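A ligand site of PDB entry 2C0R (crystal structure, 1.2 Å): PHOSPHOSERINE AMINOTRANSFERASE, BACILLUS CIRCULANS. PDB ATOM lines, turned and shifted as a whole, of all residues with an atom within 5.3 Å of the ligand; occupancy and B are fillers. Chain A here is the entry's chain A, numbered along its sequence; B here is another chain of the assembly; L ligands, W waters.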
ATOM      1  N   GLY A  75      -8.150   4.575 -19.058  1.00  0.00           N
ATOM      2  CA  GLY A  75      -8.569   5.956 -19.087  1.00  0.00           C
ATOM      3  C   GLY A  75      -7.492   6.986 -18.824  1.00  0.00           C
ATOM      4  O   GLY A  75      -7.810   8.205 -18.809  1.00  0.00           O
ATOM      5  N   GLY A  76      -6.257   6.498 -18.625  1.00  0.00           N
ATOM      6  CA  GLY A  76      -5.136   7.431 -18.430  1.00  0.00           C
ATOM      7  C   GLY A  76      -5.121   8.010 -17.031  1.00  0.00           C
ATOM      8  O   GLY A  76      -6.059   7.881 -16.231  1.00  0.00           O
ATOM      9  N   ALA A  77      -4.036   8.705 -16.746  1.00  0.00           N
ATOM     10  CA  ALA A  77      -3.993   9.467 -15.495  1.00  0.00           C
ATOM     11  C   ALA A  77      -5.134  10.480 -15.434  1.00  0.00           C
ATOM     12  O   ALA A  77      -5.626  10.795 -14.356  1.00  0.00           O
ATOM     13  CB  ALA A  77      -2.641  10.171 -15.344  1.00  0.00           C
ATOM     14  N   SER A  78      -5.544  10.985 -16.608  1.00  0.00           N
ATOM     15  CA  SER A  78      -6.637  11.973 -16.629  1.00  0.00           C
ATOM     16  C   SER A  78      -7.904  11.417 -15.983  1.00  0.00           C
ATOM     17  O   SER A  78      -8.691  12.128 -15.329  1.00  0.00           O
ATOM     18  CB  SER A  78      -6.958  12.493 -18.011  1.00  0.00           C
ATOM     19  OG  SER A  78      -5.818  13.111 -18.598  1.00  0.00           O
ATOM     20  N   THR A  79      -8.184  10.116 -16.181  1.00  0.00           N
ATOM     21  CA  THR A  79      -9.368   9.595 -15.526  1.00  0.00           C
ATOM     22  C   THR A  79      -9.163   9.522 -14.029  1.00  0.00           C
ATOM     23  O   THR A  79     -10.112   9.727 -13.275  1.00  0.00           O
ATOM     24  CB  THR A  79      -9.640   8.192 -16.095  1.00  0.00           C
ATOM     25  OG1 THR A  79     -10.131   8.452 -17.421  1.00  0.00           O
ATOM     26  CG2 THR A  79     -10.692   7.455 -15.292  1.00  0.00           C
ATOM     27  N   PHE A  81      -7.679  11.771 -12.265  1.00  0.00           N
ATOM     28  CA  PHE A  81      -7.968  13.105 -11.743  1.00  0.00           C
ATOM     29  C   PHE A  81      -9.418  13.184 -11.246  1.00  0.00           C
ATOM     30  O   PHE A  81      -9.682  13.884 -10.285  1.00  0.00           O
ATOM     31  CB  PHE A  81      -7.815  14.152 -12.839  1.00  0.00           C
ATOM     32  CG  PHE A  81      -6.389  14.339 -13.324  1.00  0.00           C
ATOM     33  CD1 PHE A  81      -6.192  15.001 -14.532  1.00  0.00           C
ATOM     34  CD2 PHE A  81      -5.311  13.828 -12.626  1.00  0.00           C
ATOM     35  CE1 PHE A  81      -4.885  15.146 -15.031  1.00  0.00           C
ATOM     36  CE2 PHE A  81      -4.003  14.031 -13.098  1.00  0.00           C
ATOM     37  CZ  PHE A  81      -3.827  14.712 -14.274  1.00  0.00           C
ATOM     38  N   TRP A 103       0.169  19.844 -14.751  1.00  0.00           N
ATOM     39  CA  TRP A 103      -0.602  18.626 -14.429  1.00  0.00           C
ATOM     40  C   TRP A 103      -1.287  18.723 -13.060  1.00  0.00           C
ATOM     41  O   TRP A 103      -2.365  18.156 -12.897  1.00  0.00           O
ATOM     42  CB  TRP A 103       0.326  17.428 -14.570  1.00  0.00           C
ATOM     43  CG  TRP A 103       0.563  17.139 -16.033  1.00  0.00           C
ATOM     44  CD1 TRP A 103       1.731  17.185 -16.715  1.00  0.00           C
ATOM     45  CD2 TRP A 103      -0.447  16.752 -16.972  1.00  0.00           C
ATOM     46  NE1 TRP A 103       1.527  16.844 -18.041  1.00  0.00           N
ATOM     47  CE2 TRP A 103       0.197  16.575 -18.219  1.00  0.00           C
ATOM     48  CE3 TRP A 103      -1.828  16.541 -16.894  1.00  0.00           C
ATOM     49  CZ2 TRP A 103      -0.503  16.201 -19.366  1.00  0.00           C
ATOM     50  CZ3 TRP A 103      -2.532  16.155 -18.035  1.00  0.00           C
ATOM     51  CH2 TRP A 103      -1.871  15.993 -19.252  1.00  0.00           C
ATOM     52  N   THR A 149       1.840  16.195  -7.533  1.00  0.00           N
ATOM     53  CA  THR A 149       2.372  15.724  -8.804  1.00  0.00           C
ATOM     54  C   THR A 149       3.856  15.577  -8.620  1.00  0.00           C
ATOM     55  O   THR A 149       4.539  16.596  -8.396  1.00  0.00           O
ATOM     56  CB  THR A 149       2.028  16.762  -9.891  1.00  0.00           C
ATOM     57  OG1 THR A 149       0.624  17.065  -9.758  1.00  0.00           O
ATOM     58  CG2 THR A 149       2.277  16.238 -11.278  1.00  0.00           C
ATOM     59  N   ASN A 151       6.277  14.724 -10.650  1.00  0.00           N
ATOM     60  CA  ASN A 151       7.101  15.291 -11.718  1.00  0.00           C
ATOM     61  C   ASN A 151       6.180  16.043 -12.643  1.00  0.00           C
ATOM     62  O   ASN A 151       5.257  15.407 -13.205  1.00  0.00           O
ATOM     63  CB  ASN A 151       7.826  14.149 -12.442  1.00  0.00           C
ATOM     64  CG  ASN A 151       8.814  14.679 -13.501  1.00  0.00           C
ATOM     65  OD1 ASN A 151       9.906  15.080 -13.117  1.00  0.00           O
ATOM     66  ND2 ASN A 151       8.446  14.622 -14.756  1.00  0.00           N
ATOM     67  N   THR A 153       5.630  17.222 -15.807  1.00  0.00           N
ATOM     68  CA  THR A 153       6.142  16.841 -17.123  1.00  0.00           C
ATOM     69  C   THR A 153       6.288  17.998 -18.092  1.00  0.00           C
ATOM     70  O   THR A 153       7.197  17.945 -18.931  1.00  0.00           O
ATOM     71  CB  THR A 153       5.109  15.858 -17.756  1.00  0.00           C
ATOM     72  OG1 THR A 153       4.609  15.064 -16.663  1.00  0.00           O
ATOM     73  CG2 THR A 153       5.812  15.003 -18.781  1.00  0.00           C
ATOM     74  N   ASP A 173       0.458  11.838  -8.301  1.00  0.00           N
ATOM     75  CA  ASP A 173       0.503  11.579  -9.730  1.00  0.00           C
ATOM     76  C   ASP A 173       1.967  11.432 -10.153  1.00  0.00           C
ATOM     77  O   ASP A 173       2.655  12.425 -10.274  1.00  0.00           O
ATOM     78  CB  ASP A 173      -0.121  12.763 -10.475  1.00  0.00           C
ATOM     79  CG  ASP A 173      -0.059  12.632 -11.986  1.00  0.00           C
ATOM     80  OD1 ASP A 173       0.474  11.638 -12.509  1.00  0.00           O
ATOM     81  OD2 ASP A 173      -0.591  13.540 -12.660  1.00  0.00           O
ATOM     82  N   SER A 175       2.859   9.989 -12.988  1.00  0.00           N
ATOM     83  CA  SER A 175       2.879   9.531 -14.381  1.00  0.00           C
ATOM     84  C   SER A 175       4.234   9.645 -15.091  1.00  0.00           C
ATOM     85  O   SER A 175       4.657   8.694 -15.761  1.00  0.00           O
ATOM     86  CB  SER A 175       1.880  10.336 -15.194  1.00  0.00           C
ATOM     87  OG  SER A 175       0.537  10.073 -14.739  1.00  0.00           O
ATOM     88  N   SER A 176       4.935  10.757 -14.898  1.00  0.00           N
ATOM     89  CA  SER A 176       6.156  10.927 -15.665  1.00  0.00           C
ATOM     90  C   SER A 176       7.412  10.558 -14.880  1.00  0.00           C
ATOM     91  O   SER A 176       8.503  10.776 -15.432  1.00  0.00           O
ATOM     92  CB  SER A 176       6.180  12.321 -16.246  1.00  0.00           C
ATOM     93  OG  SER A 176       5.972  13.309 -15.259  1.00  0.00           O
ATOM     94  N   GLY A 194      -0.125   7.064 -15.724  1.00  0.00           N
ATOM     95  CA  GLY A 194      -0.326   6.517 -17.065  1.00  0.00           C
ATOM     96  C   GLY A 194       0.947   5.793 -17.426  1.00  0.00           C
ATOM     97  O   GLY A 194       2.042   6.279 -17.200  1.00  0.00           O
ATOM     98  N   GLN A 196       2.369   5.127 -20.213  1.00  0.00           N
ATOM     99  CA  GLN A 196       3.051   5.471 -21.459  1.00  0.00           C
ATOM    100  C   GLN A 196       4.186   6.466 -21.314  1.00  0.00           C
ATOM    101  O   GLN A 196       4.840   6.744 -22.320  1.00  0.00           O
ATOM    102  CB  GLN A 196       2.025   6.042 -22.435  1.00  0.00           C
ATOM    103  CG  GLN A 196       1.431   7.397 -22.099  1.00  0.00           C
ATOM    104  CD  GLN A 196       0.249   7.346 -21.152  1.00  0.00           C
ATOM    105  OE1 GLN A 196      -0.103   6.314 -20.543  1.00  0.00           O
ATOM    106  NE2 GLN A 196      -0.376   8.537 -21.042  1.00  0.00           N
ATOM    107  N   LYS A 197       4.409   7.030 -20.144  1.00  0.00           N
ATOM    108  CA  LYS A 197       5.468   8.010 -20.034  1.00  0.00           C
ATOM    109  C   LYS A 197       6.728   7.220 -19.685  1.00  0.00           C
ATOM    110  O   LYS A 197       7.682   7.016 -20.415  1.00  0.00           O
ATOM    111  CB  LYS A 197       5.167   9.020 -18.964  1.00  0.00           C
ATOM    112  CG  LYS A 197       4.619  10.365 -19.363  1.00  0.00           C
ATOM    113  CD  LYS A 197       3.242  10.225 -19.952  1.00  0.00           C
ATOM    114  CE  LYS A 197       2.815  11.561 -20.535  1.00  0.00           C
ATOM    115  NZ  LYS A 197       2.095  12.431 -19.583  1.00  0.00           N
ATOM    116  N   THR A 205      -3.304   2.513 -16.990  1.00  0.00           N
ATOM    117  CA  THR A 205      -2.879   3.373 -15.863  1.00  0.00           C
ATOM    118  C   THR A 205      -2.624   2.452 -14.692  1.00  0.00           C
ATOM    119  O   THR A 205      -3.474   1.607 -14.330  1.00  0.00           O
ATOM    120  CB  THR A 205      -3.995   4.384 -15.561  1.00  0.00           C
ATOM    121  OG1 THR A 205      -4.267   5.113 -16.767  1.00  0.00           O
ATOM    122  CG2 THR A 205      -3.564   5.392 -14.509  1.00  0.00           C
ATOM    123  N   ASN B 238      -6.657  13.478 -24.017  1.00  0.00           N
ATOM    124  CA  ASN B 238      -5.540  12.868 -23.298  1.00  0.00           C
ATOM    125  C   ASN B 238      -4.924  11.804 -24.195  1.00  0.00           C
ATOM    126  O   ASN B 238      -5.258  11.689 -25.376  1.00  0.00           O
ATOM    127  CB  ASN B 238      -6.008  12.314 -21.964  1.00  0.00           C
ATOM    128  CG  ASN B 238      -6.704  10.973 -22.038  1.00  0.00           C
ATOM    129  OD1 ASN B 238      -7.427  10.681 -22.984  1.00  0.00           O
ATOM    130  ND2 ASN B 238      -6.531  10.194 -20.944  1.00  0.00           N
ATOM    131  N   THR B 239      -3.999  11.032 -23.660  1.00  0.00           N
ATOM    132  CA  THR B 239      -3.313  10.059 -24.482  1.00  0.00           C
ATOM    133  C   THR B 239      -4.267   8.914 -24.801  1.00  0.00           C
ATOM    134  O   THR B 239      -4.769   8.285 -23.846  1.00  0.00           O
ATOM    135  CB  THR B 239      -2.118   9.483 -23.741  1.00  0.00           C
ATOM    136  OG1 THR B 239      -1.337  10.550 -23.218  1.00  0.00           O
ATOM    137  CG2 THR B 239      -1.259   8.724 -24.764  1.00  0.00           C
HETATM  138  N1  LIG L   1      -0.164  13.575 -15.270  1.00  0.00           N
HETATM  139  C1  LIG L   1       1.116  13.725 -15.718  1.00  0.00           C
HETATM  140  C2  LIG L   1       2.161  14.130 -14.690  1.00  0.00           C
HETATM  141  C3  LIG L   1       1.425  13.508 -17.031  1.00  0.00           C
HETATM  142  O1  LIG L   1       2.708  13.601 -17.482  1.00  0.00           O
HETATM  143  C4  LIG L   1       0.430  13.060 -17.880  1.00  0.00           C
HETATM  144  C5  LIG L   1       0.767  12.809 -19.350  1.00  0.00           C
HETATM  145  C6  LIG L   1      -0.871  12.993 -17.417  1.00  0.00           C
HETATM  146  C7  LIG L   1      -1.170  13.159 -16.105  1.00  0.00           C
HETATM  147  C8  LIG L   1      -2.023  12.659 -18.386  1.00  0.00           C
HETATM  148  O2  LIG L   1      -1.982  11.278 -18.719  1.00  0.00           O
HETATM  149  P1  LIG L   1      -3.055  10.620 -19.709  1.00  0.00           P
HETATM  150  O3  LIG L   1      -2.781   9.149 -19.654  1.00  0.00           O
HETATM  151  O4  LIG L   1      -2.751  11.239 -21.056  1.00  0.00           O
HETATM  152  O5  LIG L   1      -4.399  11.015 -19.196  1.00  0.00           O
HETATM  153  O   HOH W   1      -2.407  13.822 -21.854  1.00  0.00           O
HETATM  154  O   HOH W   2       4.484  12.754 -12.612  1.00  0.00           O
HETATM  155  O   HOH W   3      -4.202   7.579 -21.381  1.00  0.00           O
HETATM  156  O   HOH W   4       0.520  14.192 -22.439  1.00  0.00           O
HETATM  157  O   HOH W   5      -0.087   9.541 -17.468  1.00  0.00           O
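OG1 of Thr 153 is in hydrogen-bond range of OG of Ser 176, 2.6 Å away.
The side-chain carboxylate (OD1) of Asp 173 is in hydrogen-bond range of the side-chain hydroxyl (OG) of Ser 175 (2.7 Å).
The side-chain amide nitrogen (NE2) of Gln 196 is in hydrogen-bond range of the side-chain hydroxyl (OG1) of Thr 239 of chain B, 3.1 Å away.
The side-chain amide nitrogen of Asn 238 of chain B sits at hydrogen-bond distance from the backbone carbonyl oxygen of Gly 75.
N of Gly 76 lies close to OG1 of Thr 205, 3.1 Å away.
OG of Ser 175 lies within hydrogen-bond range of N of Gly 194.
The side-chain hydroxyl (OG) of Ser 176 lies within hydrogen-bond range of the side-chain amide nitrogen (ND2) of Asn 151, at 2.8 Å.
Water W3 bridges the backbone carbonyl oxygen (O) of Thr 239 of chain B (2.6 Å) and an oxygen (O3) of the ligand (2.7 Å).
Water W5 lies within hydrogen-bond range of OG of Ser 175 (2.8 Å), O2 of the ligand (2.9 Å) and N of Gly 194 (3.0 Å).
Water W2 lies within hydrogen-bond range of O of Asn 151 (2.8 Å), O of Asp 173 (3.0 Å), N of Ser 176 (3.1 Å) and N of Ser 175 (3.2 Å).
C5 of the ligand is covalently linked to NZ of Lys 197 (1.4 Å).
An oxygen (O1) of the ligand is in hydrogen-bond range of the side-chain hydroxyl of Thr 153, 2.5 Å away.
The backbone NH of Ser 78 is in hydrogen-bond range of an oxygen (O5) of the ligand (2.8 Å).
The side-chain hydroxyl (OG) of Ser 78 is in hydrogen-bond range of an oxygen (O5) of the ligand (2.6 Å).
A nitrogen (N1) of the ligand is in hydrogen-bond range of the side-chain carboxylate (OD2) of Asp 173 (2.6 Å).
N of Thr 239 of chain B is in hydrogen-bond range of O4 of the ligand (2.9 Å).
The side-chain hydroxyl (OG1) of Thr 239 of chain B lies within hydrogen-bond range of an oxygen (O4) of the ligand.
O3 of the ligand lies within hydrogen-bond range of NE2 of Gln 196, 2.8 Å away.
ND2 of Asn 238 of chain B lies within hydrogen-bond range of O5 of the ligand.
An oxygen (O3) of the ligand sits at hydrogen-bond distance from the backbone NH (N) of Ala 77, 3.2 Å away.
The indole nitrogen of Trp 103 sits close to an oxygen (O1) of the ligand (3.5 Å).
Gly 76 touches the ligand.
CZ of Phe 81 touches C7 of the ligand, 3.6 Å away.
Asn 151 touches the ligand (O to C2, 3.7 Å).
CB of Ser 175 touches C1 of the ligand (3.5 Å).
Ser 176 touches the ligand (CB to O1, 3.9 Å).
14 residues have an atom within 4 Å of the ligand: Gly 76, Ala 77, Ser 78, Phe 81, Trp 103, Asn 151, Thr 153, Asp 173, Ser 175, Ser 176, Gln 196, Lys 197, Asn 238 of chain B and Thr 239 of chain B.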
